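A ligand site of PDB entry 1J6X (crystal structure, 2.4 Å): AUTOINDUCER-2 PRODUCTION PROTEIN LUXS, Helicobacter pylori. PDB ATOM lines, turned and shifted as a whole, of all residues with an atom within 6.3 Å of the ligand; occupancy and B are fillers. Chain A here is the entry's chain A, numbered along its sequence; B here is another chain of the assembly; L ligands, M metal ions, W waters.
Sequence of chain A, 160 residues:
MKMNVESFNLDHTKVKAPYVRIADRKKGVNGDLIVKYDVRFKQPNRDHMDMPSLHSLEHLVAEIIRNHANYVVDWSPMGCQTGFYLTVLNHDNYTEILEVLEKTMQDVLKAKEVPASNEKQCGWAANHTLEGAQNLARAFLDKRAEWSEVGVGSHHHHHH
The side-chain carboxylate (OD1) of Asp 74 is in salt-bridge range of a nitrogen (N1) of the ligand, at 2.5 Å.
An oxygen (O1) of the ligand sits at hydrogen-bond distance from the backbone NH (N) of Trp 75 (2.8 Å).
The backbone carbonyl oxygen (O) of Trp 75 sits at hydrogen-bond distance from a nitrogen (N1) of the ligand (2.9 Å).
An oxygen (O1) of the ligand lies within salt-bridge range of the guanidinium group of Arg 66 (2.9 Å).
A nitrogen (N1) of the ligand sits at hydrogen-bond distance from the side-chain hydroxyl of Ser 76 (3.2 Å).
An oxygen (O2) of the ligand is in salt-bridge range of the side-chain amino group (NZ) of Lys 36 of chain B, at 3.9 Å.
OD2 of Asp 74 lies within hydrogen-bond range of OG of Ser 76 (2.5 Å).
OD1 of Asp 74 lies within salt-bridge range of NZ of Lys 36 of chain B, at 2.7 Å.
The guanidinium group (NH1) of Arg 66 lies within hydrogen-bond range of the backbone carbonyl oxygen (O) of Ala 62 (3.0 Å).
The guanidinium group (NH2) of Arg 66 sits at hydrogen-bond distance from the backbone carbonyl oxygen (O) of Val 73, 3.1 Å away.
O of Phe 8 of chain B lies close to OE1 of Gln 121 (2.9 Å).
N of Gly 79 of chain B is in hydrogen-bond range of OE1 of Glu 58.
The backbone carbonyl oxygen (O) of Val 73 lies within hydrogen-bond range of the side-chain amino group (NZ) of Lys 36 of chain B, 2.8 Å away.
CD of Glu 58 touches C5 of the ligand, at 3.8 Å.
His 59 touches the ligand (CD2 to C5, 3.8 Å).
Ala 62 touches the ligand.
CG1 of Val 5 of chain B touches O2 of the ligand (3.5 Å).
CE1 of Phe 8 of chain B touches C5 of the ligand, 3.6 Å away.
Hydrophobic or aromatic side chains that line the ligand: His 59, Ala 62, Trp 75, Val 5 of chain B and Phe 8 of chain B.
Within 4 Å of the ligand: Glu 58, His 59, Ala 62, Arg 66, Asp 74, Trp 75, Ser 76, Val 5 of chain B, Phe 8 of chain B and Lys 36 of chain B.
Water W1 bridges the side-chain carboxylate of Glu 58 and a nitrogen (N1) of the ligand.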
ATOM      1  N   HIS A  55      -2.502  -1.288  13.275  1.00  0.00           N
ATOM      2  CA  HIS A  55      -1.624  -2.400  13.496  1.00  0.00           C
ATOM      3  C   HIS A  55      -2.205  -3.678  12.893  1.00  0.00           C
ATOM      4  O   HIS A  55      -1.478  -4.447  12.243  1.00  0.00           O
ATOM      5  CB  HIS A  55      -1.397  -2.607  14.998  1.00  0.00           C
ATOM      6  CG  HIS A  55      -0.342  -3.624  15.306  1.00  0.00           C
ATOM      7  ND1 HIS A  55      -0.091  -4.100  16.580  1.00  0.00           N
ATOM      8  CD2 HIS A  55       0.554  -4.244  14.495  1.00  0.00           C
ATOM      9  CE1 HIS A  55       0.888  -4.968  16.546  1.00  0.00           C
ATOM     10  NE2 HIS A  55       1.309  -5.078  15.300  1.00  0.00           N
ATOM     11  N   GLU A  58      -2.046  -3.610   9.169  1.00  0.00           N
ATOM     12  CA  GLU A  58      -0.683  -3.848   8.704  1.00  0.00           C
ATOM     13  C   GLU A  58      -0.537  -5.371   8.516  1.00  0.00           C
ATOM     14  O   GLU A  58      -0.185  -5.836   7.434  1.00  0.00           O
ATOM     15  CB  GLU A  58       0.326  -3.376   9.763  1.00  0.00           C
ATOM     16  CG  GLU A  58       1.779  -3.551   9.386  1.00  0.00           C
ATOM     17  CD  GLU A  58       2.716  -3.313  10.570  1.00  0.00           C
ATOM     18  OE1 GLU A  58       3.883  -2.897  10.349  1.00  0.00           O
ATOM     19  OE2 GLU A  58       2.310  -3.550  11.723  1.00  0.00           O
ATOM     20  N   HIS A  59      -0.822  -6.113   9.575  1.00  0.00           N
ATOM     21  CA  HIS A  59      -0.768  -7.576   9.546  1.00  0.00           C
ATOM     22  C   HIS A  59      -1.603  -8.198   8.422  1.00  0.00           C
ATOM     23  O   HIS A  59      -1.095  -8.953   7.602  1.00  0.00           O
ATOM     24  CB  HIS A  59      -1.292  -8.171  10.852  1.00  0.00           C
ATOM     25  CG  HIS A  59      -0.277  -8.248  11.936  1.00  0.00           C
ATOM     26  ND1 HIS A  59      -0.191  -9.325  12.783  1.00  0.00           N
ATOM     27  CD2 HIS A  59       0.657  -7.359  12.347  1.00  0.00           C
ATOM     28  CE1 HIS A  59       0.756  -9.096  13.675  1.00  0.00           C
ATOM     29  NE2 HIS A  59       1.281  -7.920  13.430  1.00  0.00           N
ATOM     30  N   ALA A  62      -0.560  -7.169   4.800  1.00  0.00           N
ATOM     31  CA  ALA A  62       0.790  -7.675   4.543  1.00  0.00           C
ATOM     32  C   ALA A  62       0.802  -9.142   4.148  1.00  0.00           C
ATOM     33  O   ALA A  62       1.578  -9.568   3.301  1.00  0.00           O
ATOM     34  CB  ALA A  62       1.679  -7.460   5.776  1.00  0.00           C
ATOM     35  N   GLU A  63      -0.059  -9.932   4.791  1.00  0.00           N
ATOM     36  CA  GLU A  63      -0.157 -11.352   4.470  1.00  0.00           C
ATOM     37  C   GLU A  63      -1.090 -11.565   3.283  1.00  0.00           C
ATOM     38  O   GLU A  63      -0.775 -12.314   2.349  1.00  0.00           O
ATOM     39  CB  GLU A  63      -0.703 -12.133   5.658  1.00  0.00           C
ATOM     40  CG  GLU A  63      -0.897 -13.624   5.372  1.00  0.00           C
ATOM     41  CD  GLU A  63      -0.394 -14.494   6.519  1.00  0.00           C
ATOM     42  OE1 GLU A  63      -1.227 -14.888   7.368  1.00  0.00           O
ATOM     43  OE2 GLU A  63       0.831 -14.779   6.581  1.00  0.00           O
ATOM     44  N   ARG A  66       0.225 -10.543  -0.373  1.00  0.00           N
ATOM     45  CA  ARG A  66       1.236 -11.453  -0.925  1.00  0.00           C
ATOM     46  C   ARG A  66       0.610 -12.802  -1.341  1.00  0.00           C
ATOM     47  O   ARG A  66       1.300 -13.685  -1.851  1.00  0.00           O
ATOM     48  CB  ARG A  66       2.380 -11.691   0.085  1.00  0.00           C
ATOM     49  CG  ARG A  66       3.261 -10.474   0.386  1.00  0.00           C
ATOM     50  CD  ARG A  66       4.317 -10.789   1.459  1.00  0.00           C
ATOM     51  NE  ARG A  66       5.376  -9.784   1.537  1.00  0.00           N
ATOM     52  CZ  ARG A  66       5.351  -8.678   2.292  1.00  0.00           C
ATOM     53  NH1 ARG A  66       4.305  -8.397   3.057  1.00  0.00           N
ATOM     54  NH2 ARG A  66       6.376  -7.830   2.279  1.00  0.00           N
ATOM     55  N   VAL A  72       5.699  -8.056  -3.992  1.00  0.00           N
ATOM     56  CA  VAL A  72       5.588  -7.093  -2.898  1.00  0.00           C
ATOM     57  C   VAL A  72       6.834  -7.137  -2.019  1.00  0.00           C
ATOM     58  O   VAL A  72       7.179  -8.161  -1.452  1.00  0.00           O
ATOM     59  CB  VAL A  72       4.344  -7.349  -2.023  1.00  0.00           C
ATOM     60  CG1 VAL A  72       4.318  -6.374  -0.901  1.00  0.00           C
ATOM     61  CG2 VAL A  72       3.072  -7.260  -2.854  1.00  0.00           C
ATOM     62  N   VAL A  73       7.504  -6.004  -1.901  1.00  0.00           N
ATOM     63  CA  VAL A  73       8.697  -5.978  -1.088  1.00  0.00           C
ATOM     64  C   VAL A  73       8.299  -5.656   0.337  1.00  0.00           C
ATOM     65  O   VAL A  73       8.829  -6.240   1.266  1.00  0.00           O
ATOM     66  CB  VAL A  73       9.702  -4.912  -1.544  1.00  0.00           C
ATOM     67  CG1 VAL A  73      10.819  -4.815  -0.532  1.00  0.00           C
ATOM     68  CG2 VAL A  73      10.279  -5.274  -2.915  1.00  0.00           C
ATOM     69  N   ASP A  74       7.325  -4.768   0.498  1.00  0.00           N
ATOM     70  CA  ASP A  74       6.966  -4.340   1.833  1.00  0.00           C
ATOM     71  C   ASP A  74       5.612  -3.585   1.912  1.00  0.00           C
ATOM     72  O   ASP A  74       5.248  -2.894   0.962  1.00  0.00           O
ATOM     73  CB  ASP A  74       8.101  -3.433   2.334  1.00  0.00           C
ATOM     74  CG  ASP A  74       7.979  -3.079   3.793  1.00  0.00           C
ATOM     75  OD1 ASP A  74       8.266  -3.939   4.642  1.00  0.00           O
ATOM     76  OD2 ASP A  74       7.594  -1.923   4.079  1.00  0.00           O
ATOM     77  N   TRP A  75       4.908  -3.764   3.032  1.00  0.00           N
ATOM     78  CA  TRP A  75       3.654  -3.060   3.335  1.00  0.00           C
ATOM     79  C   TRP A  75       3.863  -2.391   4.708  1.00  0.00           C
ATOM     80  O   TRP A  75       3.774  -3.054   5.745  1.00  0.00           O
ATOM     81  CB  TRP A  75       2.455  -4.017   3.441  1.00  0.00           C
ATOM     82  CG  TRP A  75       1.172  -3.343   3.906  1.00  0.00           C
ATOM     83  CD1 TRP A  75       0.604  -3.400   5.155  1.00  0.00           C
ATOM     84  CD2 TRP A  75       0.285  -2.532   3.113  1.00  0.00           C
ATOM     85  NE1 TRP A  75      -0.566  -2.687   5.188  1.00  0.00           N
ATOM     86  CE2 TRP A  75      -0.787  -2.137   3.948  1.00  0.00           C
ATOM     87  CE3 TRP A  75       0.293  -2.105   1.781  1.00  0.00           C
ATOM     88  CZ2 TRP A  75      -1.849  -1.346   3.483  1.00  0.00           C
ATOM     89  CZ3 TRP A  75      -0.767  -1.301   1.321  1.00  0.00           C
ATOM     90  CH2 TRP A  75      -1.820  -0.941   2.173  1.00  0.00           C
ATOM     91  N   SER A  76       4.146  -1.093   4.712  1.00  0.00           N
ATOM     92  CA  SER A  76       4.423  -0.383   5.955  1.00  0.00           C
ATOM     93  C   SER A  76       3.511   0.772   6.315  1.00  0.00           C
ATOM     94  O   SER A  76       3.094   1.542   5.455  1.00  0.00           O
ATOM     95  CB  SER A  76       5.857   0.147   5.917  1.00  0.00           C
ATOM     96  OG  SER A  76       6.803  -0.873   6.169  1.00  0.00           O
ATOM     97  N   PRO A  77       3.196   0.906   7.622  1.00  0.00           N
ATOM     98  CA  PRO A  77       2.335   1.992   8.113  1.00  0.00           C
ATOM     99  C   PRO A  77       3.178   3.257   8.171  1.00  0.00           C
ATOM    100  O   PRO A  77       4.398   3.177   8.337  1.00  0.00           O
ATOM    101  CB  PRO A  77       1.958   1.523   9.519  1.00  0.00           C
ATOM    102  CG  PRO A  77       3.214   0.798   9.957  1.00  0.00           C
ATOM    103  CD  PRO A  77       3.517  -0.027   8.717  1.00  0.00           C
ATOM    104  N   GLN A 121       4.871 -13.917  17.302  1.00  0.00           N
ATOM    105  CA  GLN A 121       5.068 -13.347  15.966  1.00  0.00           C
ATOM    106  C   GLN A 121       4.793 -11.849  15.830  1.00  0.00           C
ATOM    107  O   GLN A 121       4.807 -11.306  14.723  1.00  0.00           O
ATOM    108  CB  GLN A 121       4.213 -14.109  14.948  1.00  0.00           C
ATOM    109  CG  GLN A 121       4.007 -15.578  15.266  1.00  0.00           C
ATOM    110  CD  GLN A 121       3.112 -16.260  14.258  1.00  0.00           C
ATOM    111  OE1 GLN A 121       3.572 -16.767  13.228  1.00  0.00           O
ATOM    112  NE2 GLN A 121       1.825 -16.273  14.540  1.00  0.00           N
ATOM    113  N   VAL B   5       4.839 -13.602   5.494  1.00  0.00           N
ATOM    114  CA  VAL B   5       5.586 -12.427   5.902  1.00  0.00           C
ATOM    115  C   VAL B   5       6.804 -12.840   6.700  1.00  0.00           C
ATOM    116  O   VAL B   5       6.696 -13.632   7.615  1.00  0.00           O
ATOM    117  CB  VAL B   5       4.675 -11.530   6.768  1.00  0.00           C
ATOM    118  CG1 VAL B   5       5.478 -10.342   7.312  1.00  0.00           C
ATOM    119  CG2 VAL B   5       3.473 -11.077   5.943  1.00  0.00           C
ATOM    120  N   GLU B   6       7.954 -12.291   6.370  1.00  0.00           N
ATOM    121  CA  GLU B   6       9.195 -12.652   7.048  1.00  0.00           C
ATOM    122  C   GLU B   6       9.184 -12.530   8.576  1.00  0.00           C
ATOM    123  O   GLU B   6       9.523 -13.495   9.273  1.00  0.00           O
ATOM    124  CB  GLU B   6      10.369 -11.841   6.502  1.00  0.00           C
ATOM    125  CG  GLU B   6      11.738 -12.300   7.023  1.00  0.00           C
ATOM    126  CD  GLU B   6      12.039 -11.884   8.481  1.00  0.00           C
ATOM    127  OE1 GLU B   6      12.808 -12.638   9.143  1.00  0.00           O
ATOM    128  OE2 GLU B   6      11.546 -10.822   8.940  1.00  0.00           O
ATOM    129  N   SER B   7       8.808 -11.371   9.089  1.00  0.00           N
ATOM    130  CA  SER B   7       8.812 -11.189  10.532  1.00  0.00           C
ATOM    131  C   SER B   7       7.880 -12.123  11.306  1.00  0.00           C
ATOM    132  O   SER B   7       8.069 -12.307  12.517  1.00  0.00           O
ATOM    133  CB  SER B   7       8.525  -9.742  10.886  1.00  0.00           C
ATOM    134  OG  SER B   7       7.135  -9.484  10.874  1.00  0.00           O
ATOM    135  N   PHE B   8       6.881 -12.707  10.654  1.00  0.00           N
ATOM    136  CA  PHE B   8       5.982 -13.616  11.345  1.00  0.00           C
ATOM    137  C   PHE B   8       6.687 -14.940  11.612  1.00  0.00           C
ATOM    138  O   PHE B   8       6.159 -15.827  12.274  1.00  0.00           O
ATOM    139  CB  PHE B   8       4.704 -13.868  10.522  1.00  0.00           C
ATOM    140  CG  PHE B   8       3.813 -12.668  10.372  1.00  0.00           C
ATOM    141  CD1 PHE B   8       4.106 -11.460  11.009  1.00  0.00           C
ATOM    142  CD2 PHE B   8       2.645 -12.747   9.611  1.00  0.00           C
ATOM    143  CE1 PHE B   8       3.255 -10.362  10.894  1.00  0.00           C
ATOM    144  CE2 PHE B   8       1.788 -11.653   9.489  1.00  0.00           C
ATOM    145  CZ  PHE B   8       2.101 -10.468  10.134  1.00  0.00           C
ATOM    146  N   LYS B  36      16.852  -5.928   3.884  1.00  0.00           N
ATOM    147  CA  LYS B  36      15.960  -5.353   4.862  1.00  0.00           C
ATOM    148  C   LYS B  36      16.474  -5.641   6.278  1.00  0.00           C
ATOM    149  O   LYS B  36      16.806  -6.784   6.614  1.00  0.00           O
ATOM    150  CB  LYS B  36      14.597  -5.992   4.682  1.00  0.00           C
ATOM    151  CG  LYS B  36      13.464  -5.058   4.445  1.00  0.00           C
ATOM    152  CD  LYS B  36      12.278  -5.888   3.984  1.00  0.00           C
ATOM    153  CE  LYS B  36      10.984  -5.151   4.230  1.00  0.00           C
ATOM    154  NZ  LYS B  36       9.852  -6.026   3.897  1.00  0.00           N
ATOM    155  N   GLY B  79       4.215  -1.308  12.922  1.00  0.00           N
ATOM    156  CA  GLY B  79       2.938  -1.018  13.533  1.00  0.00           C
ATOM    157  C   GLY B  79       2.940  -1.400  15.002  1.00  0.00           C
ATOM    158  O   GLY B  79       2.160  -0.866  15.805  1.00  0.00           O
ATOM    159  N   CYS B  80       3.815  -2.315  15.378  1.00  0.00           N
ATOM    160  CA  CYS B  80       3.896  -2.761  16.769  1.00  0.00           C
ATOM    161  C   CYS B  80       4.615  -1.749  17.655  1.00  0.00           C
ATOM    162  O   CYS B  80       4.797  -1.971  18.848  1.00  0.00           O
ATOM    163  CB  CYS B  80       4.596  -4.120  16.840  1.00  0.00           C
ATOM    164  SG  CYS B  80       6.240  -4.180  16.076  1.00  0.00           S
ATOM    165  N   TYR B  85      11.885  -0.664  10.109  1.00  0.00           N
ATOM    166  CA  TYR B  85      12.509  -1.449   9.055  1.00  0.00           C
ATOM    167  C   TYR B  85      13.324  -0.477   8.208  1.00  0.00           C
ATOM    168  O   TYR B  85      12.883   0.632   7.883  1.00  0.00           O
ATOM    169  CB  TYR B  85      11.468  -2.144   8.180  1.00  0.00           C
ATOM    170  CG  TYR B  85      10.986  -3.474   8.727  1.00  0.00           C
ATOM    171  CD1 TYR B  85      11.860  -4.547   8.882  1.00  0.00           C
ATOM    172  CD2 TYR B  85       9.656  -3.654   9.076  1.00  0.00           C
ATOM    173  CE1 TYR B  85      11.417  -5.781   9.375  1.00  0.00           C
ATOM    174  CE2 TYR B  85       9.198  -4.872   9.576  1.00  0.00           C
ATOM    175  CZ  TYR B  85      10.080  -5.930   9.729  1.00  0.00           C
ATOM    176  OH  TYR B  85       9.628  -7.122  10.254  1.00  0.00           O
HETATM  177  N1  LIG L   1       6.446  -4.065   6.295  1.00  0.00           N
HETATM  178  C1  LIG L   1       6.379  -5.478   6.747  1.00  0.00           C
HETATM  179  C2  LIG L   1       6.280  -6.431   5.541  1.00  0.00           C
HETATM  180  O1  LIG L   1       5.730  -6.021   4.500  1.00  0.00           O
HETATM  181  C3  LIG L   1       5.151  -5.634   7.656  1.00  0.00           C
HETATM  182  C4  LIG L   1       4.903  -7.026   8.162  1.00  0.00           C
HETATM  183  S1  LIG L   1       3.413  -7.144   9.186  1.00  0.00           S
HETATM  184  C5  LIG L   1       4.085  -6.821  10.809  1.00  0.00           C
HETATM  185  O2  LIG L   1       6.755  -7.578   5.646  1.00  0.00           O
HETATM  186 ZN    ZN M   1       2.412  -6.819  15.010  1.00  0.00          ZN
HETATM  187  O   HOH W   1       6.156  -3.095   9.294  1.00  0.00           O
